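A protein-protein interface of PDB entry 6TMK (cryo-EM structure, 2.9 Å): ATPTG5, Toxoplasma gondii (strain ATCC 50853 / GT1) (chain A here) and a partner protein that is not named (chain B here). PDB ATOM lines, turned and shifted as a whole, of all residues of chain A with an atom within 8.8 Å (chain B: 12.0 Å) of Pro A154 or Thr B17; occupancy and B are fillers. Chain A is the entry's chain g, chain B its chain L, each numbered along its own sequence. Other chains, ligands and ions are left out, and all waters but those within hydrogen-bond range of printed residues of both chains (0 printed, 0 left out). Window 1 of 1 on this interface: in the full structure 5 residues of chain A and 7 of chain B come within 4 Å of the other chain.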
ATOM      1  N   ASP A 149      -2.090  28.642  32.917  1.00  0.00           N
ATOM      2  CA  ASP A 149      -3.123  28.914  31.928  1.00  0.00           C
ATOM      3  C   ASP A 149      -4.329  29.561  32.595  1.00  0.00           C
ATOM      4  O   ASP A 149      -4.934  28.979  33.501  1.00  0.00           O
ATOM      5  CB  ASP A 149      -3.536  27.625  31.217  1.00  0.00           C
ATOM      6  CG  ASP A 149      -3.891  27.847  29.763  1.00  0.00           C
ATOM      7  OD1 ASP A 149      -4.100  29.010  29.366  1.00  0.00           O
ATOM      8  OD2 ASP A 149      -3.964  26.850  29.016  1.00  0.00           O
ATOM      9  N   ASP A 150      -4.672  30.763  32.141  1.00  0.00           N
ATOM     10  CA  ASP A 150      -5.903  31.416  32.551  1.00  0.00           C
ATOM     11  C   ASP A 150      -7.115  30.915  31.778  1.00  0.00           C
ATOM     12  O   ASP A 150      -8.245  31.260  32.139  1.00  0.00           O
ATOM     13  CB  ASP A 150      -5.772  32.925  32.368  1.00  0.00           C
ATOM     14  CG  ASP A 150      -4.768  33.546  33.316  1.00  0.00           C
ATOM     15  OD1 ASP A 150      -4.971  33.462  34.545  1.00  0.00           O
ATOM     16  OD2 ASP A 150      -3.775  34.125  32.831  1.00  0.00           O
ATOM     17  N   LEU A 151      -6.908  30.123  30.729  1.00  0.00           N
ATOM     18  CA  LEU A 151      -7.981  29.607  29.895  1.00  0.00           C
ATOM     19  C   LEU A 151      -8.341  28.166  30.216  1.00  0.00           C
ATOM     20  O   LEU A 151      -9.186  27.582  29.533  1.00  0.00           O
ATOM     21  CB  LEU A 151      -7.586  29.708  28.428  1.00  0.00           C
ATOM     22  CG  LEU A 151      -7.641  31.074  27.765  1.00  0.00           C
ATOM     23  CD1 LEU A 151      -7.020  30.983  26.399  1.00  0.00           C
ATOM     24  CD2 LEU A 151      -9.059  31.544  27.659  1.00  0.00           C
ATOM     25  N   HIS A 152      -7.737  27.587  31.250  1.00  0.00           N
ATOM     26  CA  HIS A 152      -7.885  26.160  31.504  1.00  0.00           C
ATOM     27  C   HIS A 152      -9.333  25.798  31.801  1.00  0.00           C
ATOM     28  O   HIS A 152      -9.937  24.968  31.110  1.00  0.00           O
ATOM     29  CB  HIS A 152      -6.969  25.759  32.657  1.00  0.00           C
ATOM     30  CG  HIS A 152      -7.219  24.380  33.175  1.00  0.00           C
ATOM     31  ND1 HIS A 152      -7.123  23.260  32.381  1.00  0.00           N
ATOM     32  CD2 HIS A 152      -7.549  23.941  34.409  1.00  0.00           C
ATOM     33  CE1 HIS A 152      -7.394  22.189  33.104  1.00  0.00           C
ATOM     34  NE2 HIS A 152      -7.656  22.574  34.339  1.00  0.00           N
ATOM     35  N   TYR A 153      -9.910  26.427  32.808  1.00  0.00           N
ATOM     36  CA  TYR A 153     -11.255  26.112  33.259  1.00  0.00           C
ATOM     37  C   TYR A 153     -12.310  26.602  32.275  1.00  0.00           C
ATOM     38  O   TYR A 153     -13.287  25.889  32.018  1.00  0.00           O
ATOM     39  CB  TYR A 153     -11.493  26.712  34.642  1.00  0.00           C
ATOM     40  CG  TYR A 153     -10.887  25.911  35.765  1.00  0.00           C
ATOM     41  CD1 TYR A 153     -11.398  24.675  36.112  1.00  0.00           C
ATOM     42  CD2 TYR A 153      -9.804  26.390  36.477  1.00  0.00           C
ATOM     43  CE1 TYR A 153     -10.851  23.943  37.132  1.00  0.00           C
ATOM     44  CE2 TYR A 153      -9.252  25.661  37.498  1.00  0.00           C
ATOM     45  CZ  TYR A 153      -9.780  24.440  37.822  1.00  0.00           C
ATOM     46  OH  TYR A 153      -9.230  23.710  38.844  1.00  0.00           O
ATOM     47  N   PRO A 154     -12.167  27.801  31.713  1.00  0.00           N
ATOM     48  CA  PRO A 154     -13.095  28.197  30.642  1.00  0.00           C
ATOM     49  C   PRO A 154     -13.109  27.233  29.472  1.00  0.00           C
ATOM     50  O   PRO A 154     -14.184  26.864  28.984  1.00  0.00           O
ATOM     51  CB  PRO A 154     -12.570  29.576  30.240  1.00  0.00           C
ATOM     52  CG  PRO A 154     -11.915  30.099  31.430  1.00  0.00           C
ATOM     53  CD  PRO A 154     -11.362  28.939  32.185  1.00  0.00           C
ATOM     54  N   ARG A 155     -11.935  26.824  28.996  1.00  0.00           N
ATOM     55  CA  ARG A 155     -11.856  25.866  27.901  1.00  0.00           C
ATOM     56  C   ARG A 155     -12.492  24.536  28.277  1.00  0.00           C
ATOM     57  O   ARG A 155     -13.231  23.940  27.485  1.00  0.00           O
ATOM     58  CB  ARG A 155     -10.397  25.671  27.518  1.00  0.00           C
ATOM     59  CG  ARG A 155     -10.142  24.615  26.484  1.00  0.00           C
ATOM     60  CD  ARG A 155      -8.779  24.812  25.900  1.00  0.00           C
ATOM     61  NE  ARG A 155      -7.793  25.065  26.945  1.00  0.00           N
ATOM     62  CZ  ARG A 155      -6.804  25.946  26.862  1.00  0.00           C
ATOM     63  NH1 ARG A 155      -6.638  26.682  25.778  1.00  0.00           N
ATOM     64  NH2 ARG A 155      -5.971  26.085  27.878  1.00  0.00           N
ATOM     65  N   GLN A 156     -12.189  24.040  29.478  1.00  0.00           N
ATOM     66  CA  GLN A 156     -12.777  22.793  29.949  1.00  0.00           C
ATOM     67  C   GLN A 156     -14.299  22.868  29.953  1.00  0.00           C
ATOM     68  O   GLN A 156     -14.983  21.962  29.460  1.00  0.00           O
ATOM     69  CB  GLN A 156     -12.232  22.491  31.343  1.00  0.00           C
ATOM     70  CG  GLN A 156     -12.379  21.069  31.807  1.00  0.00           C
ATOM     71  CD  GLN A 156     -11.494  20.783  32.997  1.00  0.00           C
ATOM     72  OE1 GLN A 156     -11.089  21.696  33.712  1.00  0.00           O
ATOM     73  NE2 GLN A 156     -11.175  19.514  33.210  1.00  0.00           N
ATOM     74  N   MET A 157     -14.844  23.954  30.502  1.00  0.00           N
ATOM     75  CA  MET A 157     -16.291  24.117  30.557  1.00  0.00           C
ATOM     76  C   MET A 157     -16.884  24.188  29.162  1.00  0.00           C
ATOM     77  O   MET A 157     -17.926  23.584  28.893  1.00  0.00           O
ATOM     78  CB  MET A 157     -16.652  25.364  31.355  1.00  0.00           C
ATOM     79  CG  MET A 157     -18.143  25.611  31.478  1.00  0.00           C
ATOM     80  SD  MET A 157     -19.048  24.256  32.234  1.00  0.00           S
ATOM     81  CE  MET A 157     -18.330  24.275  33.862  1.00  0.00           C
ATOM     82  N   LEU A 158     -16.246  24.936  28.269  1.00  0.00           N
ATOM     83  CA  LEU A 158     -16.760  25.072  26.917  1.00  0.00           C
ATOM     84  C   LEU A 158     -16.800  23.722  26.220  1.00  0.00           C
ATOM     85  O   LEU A 158     -17.803  23.359  25.597  1.00  0.00           O
ATOM     86  CB  LEU A 158     -15.894  26.054  26.136  1.00  0.00           C
ATOM     87  CG  LEU A 158     -16.328  26.346  24.710  1.00  0.00           C
ATOM     88  CD1 LEU A 158     -17.630  27.092  24.715  1.00  0.00           C
ATOM     89  CD2 LEU A 158     -15.272  27.147  24.025  1.00  0.00           C
ATOM     90  N   LEU A 159     -15.718  22.958  26.331  1.00  0.00           N
ATOM     91  CA  LEU A 159     -15.663  21.655  25.685  1.00  0.00           C
ATOM     92  C   LEU A 159     -16.715  20.714  26.253  1.00  0.00           C
ATOM     93  O   LEU A 159     -17.382  19.995  25.500  1.00  0.00           O
ATOM     94  CB  LEU A 159     -14.273  21.057  25.851  1.00  0.00           C
ATOM     95  CG  LEU A 159     -13.143  21.824  25.176  1.00  0.00           C
ATOM     96  CD1 LEU A 159     -11.810  21.380  25.729  1.00  0.00           C
ATOM     97  CD2 LEU A 159     -13.184  21.636  23.690  1.00  0.00           C
ATOM     98  N   CYS A 160     -16.884  20.699  27.574  1.00  0.00           N
ATOM     99  CA  CYS A 160     -17.850  19.775  28.157  1.00  0.00           C
ATOM    100  C   CYS A 160     -19.282  20.177  27.819  1.00  0.00           C
ATOM    101  O   CYS A 160     -20.113  19.318  27.493  1.00  0.00           O
ATOM    102  CB  CYS A 160     -17.656  19.696  29.667  1.00  0.00           C
ATOM    103  SG  CYS A 160     -16.193  18.781  30.181  1.00  0.00           S
ATOM    104  N   ARG A 161     -19.593  21.473  27.871  1.00  0.00           N
ATOM    105  CA  ARG A 161     -20.929  21.914  27.499  1.00  0.00           C
ATOM    106  C   ARG A 161     -21.205  21.683  26.022  1.00  0.00           C
ATOM    107  O   ARG A 161     -22.362  21.481  25.638  1.00  0.00           O
ATOM    108  CB  ARG A 161     -21.113  23.390  27.838  1.00  0.00           C
ATOM    109  CG  ARG A 161     -21.090  23.719  29.317  1.00  0.00           C
ATOM    110  CD  ARG A 161     -22.114  22.934  30.101  1.00  0.00           C
ATOM    111  NE  ARG A 161     -23.466  23.135  29.598  1.00  0.00           N
ATOM    112  CZ  ARG A 161     -24.242  24.159  29.929  1.00  0.00           C
ATOM    113  NH1 ARG A 161     -23.801  25.090  30.763  1.00  0.00           N
ATOM    114  NH2 ARG A 161     -25.458  24.254  29.417  1.00  0.00           N
ATOM    115  N   GLY A 162     -20.173  21.715  25.179  1.00  0.00           N
ATOM    116  CA  GLY A 162     -20.371  21.355  23.791  1.00  0.00           C
ATOM    117  C   GLY A 162     -20.567  19.869  23.596  1.00  0.00           C
ATOM    118  O   GLY A 162     -21.314  19.449  22.708  1.00  0.00           O
ATOM    119  N   CYS A 170     -20.128  19.209  34.623  1.00  0.00           N
ATOM    120  CA  CYS A 170     -18.858  19.836  34.281  1.00  0.00           C
ATOM    121  C   CYS A 170     -18.053  20.170  35.527  1.00  0.00           C
ATOM    122  O   CYS A 170     -16.838  19.959  35.563  1.00  0.00           O
ATOM    123  CB  CYS A 170     -19.103  21.093  33.452  1.00  0.00           C
ATOM    124  SG  CYS A 170     -19.802  20.801  31.819  1.00  0.00           S
ATOM    125  N   ALA A 174     -14.467  18.598  36.450  1.00  0.00           N
ATOM    126  CA  ALA A 174     -13.363  19.537  36.323  1.00  0.00           C
ATOM    127  C   ALA A 174     -12.179  19.110  37.178  1.00  0.00           C
ATOM    128  O   ALA A 174     -12.341  18.596  38.287  1.00  0.00           O
ATOM    129  CB  ALA A 174     -13.806  20.940  36.723  1.00  0.00           C
ATOM    130  N   ALA B  10      -6.054  39.298  33.606  1.00  0.00           N
ATOM    131  CA  ALA B  10      -5.500  38.065  33.075  1.00  0.00           C
ATOM    132  C   ALA B  10      -4.293  38.353  32.196  1.00  0.00           C
ATOM    133  O   ALA B  10      -4.248  39.356  31.480  1.00  0.00           O
ATOM    134  CB  ALA B  10      -6.561  37.317  32.276  1.00  0.00           C
ATOM    135  N   ASN B  11      -3.308  37.457  32.250  1.00  0.00           N
ATOM    136  CA  ASN B  11      -2.134  37.603  31.401  1.00  0.00           C
ATOM    137  C   ASN B  11      -2.390  37.008  30.027  1.00  0.00           C
ATOM    138  O   ASN B  11      -2.034  37.604  29.007  1.00  0.00           O
ATOM    139  CB  ASN B  11      -0.923  36.949  32.060  1.00  0.00           C
ATOM    140  CG  ASN B  11      -0.869  37.197  33.544  1.00  0.00           C
ATOM    141  OD1 ASN B  11      -1.237  38.268  34.020  1.00  0.00           O
ATOM    142  ND2 ASN B  11      -0.412  36.206  34.289  1.00  0.00           N
ATOM    143  N   VAL B  12      -3.007  35.842  29.992  1.00  0.00           N
ATOM    144  CA  VAL B  12      -3.476  35.253  28.749  1.00  0.00           C
ATOM    145  C   VAL B  12      -4.807  35.890  28.385  1.00  0.00           C
ATOM    146  O   VAL B  12      -5.626  36.197  29.258  1.00  0.00           O
ATOM    147  CB  VAL B  12      -3.598  33.726  28.887  1.00  0.00           C
ATOM    148  CG1 VAL B  12      -4.241  33.138  27.658  1.00  0.00           C
ATOM    149  CG2 VAL B  12      -2.244  33.107  29.129  1.00  0.00           C
ATOM    150  N   ALA B  13      -5.028  36.091  27.095  1.00  0.00           N
ATOM    151  CA  ALA B  13      -6.212  36.799  26.634  1.00  0.00           C
ATOM    152  C   ALA B  13      -7.418  35.871  26.650  1.00  0.00           C
ATOM    153  O   ALA B  13      -7.419  34.834  25.980  1.00  0.00           O
ATOM    154  CB  ALA B  13      -5.984  37.347  25.231  1.00  0.00           C
ATOM    155  N   VAL B  14      -8.438  36.242  27.414  1.00  0.00           N
ATOM    156  CA  VAL B  14      -9.745  35.607  27.335  1.00  0.00           C
ATOM    157  C   VAL B  14     -10.593  36.474  26.419  1.00  0.00           C
ATOM    158  O   VAL B  14     -10.783  37.668  26.680  1.00  0.00           O
ATOM    159  CB  VAL B  14     -10.389  35.454  28.722  1.00  0.00           C
ATOM    160  CG1 VAL B  14      -9.588  34.504  29.580  1.00  0.00           C
ATOM    161  CG2 VAL B  14     -10.532  36.799  29.424  1.00  0.00           C
ATOM    162  N   SER B  15     -11.072  35.890  25.325  1.00  0.00           N
ATOM    163  CA  SER B  15     -11.889  36.619  24.363  1.00  0.00           C
ATOM    164  C   SER B  15     -13.379  36.430  24.623  1.00  0.00           C
ATOM    165  O   SER B  15     -14.081  37.384  24.970  1.00  0.00           O
ATOM    166  CB  SER B  15     -11.504  36.181  22.942  1.00  0.00           C
ATOM    167  OG  SER B  15     -11.798  34.817  22.716  1.00  0.00           O
ATOM    168  N   PHE B  16     -13.869  35.201  24.479  1.00  0.00           N
ATOM    169  CA  PHE B  16     -15.262  34.885  24.757  1.00  0.00           C
ATOM    170  C   PHE B  16     -15.388  33.511  25.397  1.00  0.00           C
ATOM    171  O   PHE B  16     -16.510  33.028  25.579  1.00  0.00           O
ATOM    172  CB  PHE B  16     -16.101  34.930  23.480  1.00  0.00           C
ATOM    173  CG  PHE B  16     -15.447  34.274  22.308  1.00  0.00           C
ATOM    174  CD1 PHE B  16     -15.479  32.904  22.168  1.00  0.00           C
ATOM    175  CD2 PHE B  16     -14.817  35.020  21.336  1.00  0.00           C
ATOM    176  CE1 PHE B  16     -14.887  32.294  21.099  1.00  0.00           C
ATOM    177  CE2 PHE B  16     -14.222  34.408  20.262  1.00  0.00           C
ATOM    178  CZ  PHE B  16     -14.260  33.045  20.144  1.00  0.00           C
ATOM    179  N   THR B  17     -14.269  32.880  25.743  1.00  0.00           N
ATOM    180  CA  THR B  17     -14.286  31.506  26.213  1.00  0.00           C
ATOM    181  C   THR B  17     -15.073  31.361  27.506  1.00  0.00           C
ATOM    182  O   THR B  17     -15.661  30.304  27.760  1.00  0.00           O
ATOM    183  CB  THR B  17     -12.845  31.041  26.403  1.00  0.00           C
ATOM    184  OG1 THR B  17     -12.078  31.416  25.255  1.00  0.00           O
ATOM    185  CG2 THR B  17     -12.778  29.548  26.566  1.00  0.00           C
ATOM    186  N   ALA B  18     -15.095  32.402  28.331  1.00  0.00           N
ATOM    187  CA  ALA B  18     -15.785  32.378  29.610  1.00  0.00           C
ATOM    188  C   ALA B  18     -17.247  32.776  29.513  1.00  0.00           C
ATOM    189  O   ALA B  18     -17.922  32.845  30.543  1.00  0.00           O
ATOM    190  CB  ALA B  18     -15.078  33.302  30.596  1.00  0.00           C
ATOM    191  N   ALA B  19     -17.753  33.038  28.315  1.00  0.00           N
ATOM    192  CA  ALA B  19     -19.130  33.462  28.182  1.00  0.00           C
ATOM    193  C   ALA B  19     -20.079  32.322  28.546  1.00  0.00           C
ATOM    194  O   ALA B  19     -19.744  31.147  28.382  1.00  0.00           O
ATOM    195  CB  ALA B  19     -19.405  33.927  26.761  1.00  0.00           C
ATOM    196  N   PRO B  20     -21.270  32.645  29.041  1.00  0.00           N
ATOM    197  CA  PRO B  20     -22.208  31.591  29.432  1.00  0.00           C
ATOM    198  C   PRO B  20     -22.747  30.831  28.233  1.00  0.00           C
ATOM    199  O   PRO B  20     -23.031  31.409  27.182  1.00  0.00           O
ATOM    200  CB  PRO B  20     -23.317  32.358  30.156  1.00  0.00           C
ATOM    201  CG  PRO B  20     -23.224  33.734  29.644  1.00  0.00           C
ATOM    202  CD  PRO B  20     -21.784  33.980  29.375  1.00  0.00           C
ATOM    203  N   ALA B  21     -22.877  29.519  28.402  1.00  0.00           N
ATOM    204  CA  ALA B  21     -23.457  28.652  27.393  1.00  0.00           C
ATOM    205  C   ALA B  21     -24.895  28.284  27.710  1.00  0.00           C
ATOM    206  O   ALA B  21     -25.448  27.380  27.079  1.00  0.00           O
ATOM    207  CB  ALA B  21     -22.618  27.387  27.250  1.00  0.00           C
ATOM    208  N   GLU B  22     -25.512  28.967  28.673  1.00  0.00           N
ATOM    209  CA  GLU B  22     -26.856  28.674  29.106  1.00  0.00           C
ATOM    210  C   GLU B  22     -27.505  29.987  29.508  1.00  0.00           C
ATOM    211  O   GLU B  22     -26.833  30.837  30.109  1.00  0.00           O
ATOM    212  CB  GLU B  22     -26.866  27.694  30.283  1.00  0.00           C
ATOM    213  CG  GLU B  22     -28.204  27.030  30.535  1.00  0.00           C
ATOM    214  CD  GLU B  22     -28.126  25.943  31.587  1.00  0.00           C
ATOM    215  OE1 GLU B  22     -29.032  25.083  31.622  1.00  0.00           O
ATOM    216  OE2 GLU B  22     -27.162  25.946  32.382  1.00  0.00           O
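N of Asn B11 lies within hydrogen-bond range of OD2 of Asp A150, at 3.4 Å. The backbone NH of Val B12 sits at hydrogen-bond distance from the side-chain carboxylate of Asp A150 (3.4 Å). The side-chain carboxylate (OE2) of Glu B22 lies within salt-bridge range of the guanidinium group (NH2) of Arg A161, 3.8 Å away.
The backbone NH (N) of Leu A151 lies close to the side-chain carboxylate (OD1) of Asp A149 (3.3 Å). OD2 of Asp A149 is in salt-bridge range of NH2 of Arg A155 (2.4 Å).
Among the printed residues, pairs that only touch across the chains: Leu A151 with Val B12, Leu A151 with Ala B13, Leu A151 with Val B14, Leu A151 with Thr B17, Pro A154 with Thr B17, Arg A155 with Thr B17 and Arg A161 with Ala B21.
Asp A149 touches none of the printed residues of chain B. Of the printed residues of chain B, Asp A150 touches Asn B11 (3.4 Å) and Val B12 (3.4 Å). Of chain B, only Val B12 (3.7 Å), Ala B13 (3.9 Å), Val B14 (3.6 Å) and Thr B17 (3.9 Å) come within 4 Å of Leu A151. No residue of chain B comes within 4 Å of His A152. Printed residues of chain A within 4 Å of Ala B13: Leu A151 (3.9 Å). Of the printed residues of chain A, Val B14 touches Leu A151 (3.6 Å). Of chain A, only Leu A151, Pro A154 and Arg A155 come within 4 Å of Thr B17. Ala B18 touches none of the printed residues of chain A. Of the printed residues of chain A, Glu B22 touches Arg A161 (3.8 Å). The nearest residue of chain B that does not touch Pro A154 is Ala B18 (4.2 Å). The nearest printed residue of chain A that does not touch Val B14 is Asp A150 (4.3 Å).
Of the 16 printed residues of chain A, 5 touch a printed residue of chain B. Hydrophobic or aromatic side chains of chain A that line the printed part of chain B: Leu A151 and Pro A154. Along chain A the printed residues that touch a printed residue of chain B span positions 150 to 161. Of the 13 printed residues of chain B, 7 touch a printed residue of chain A. Among the printed residues, Asp or Glu carboxylates within 4 Å of a Lys or Arg side-chain nitrogen of the other chain: Arg A161 with Glu B22.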
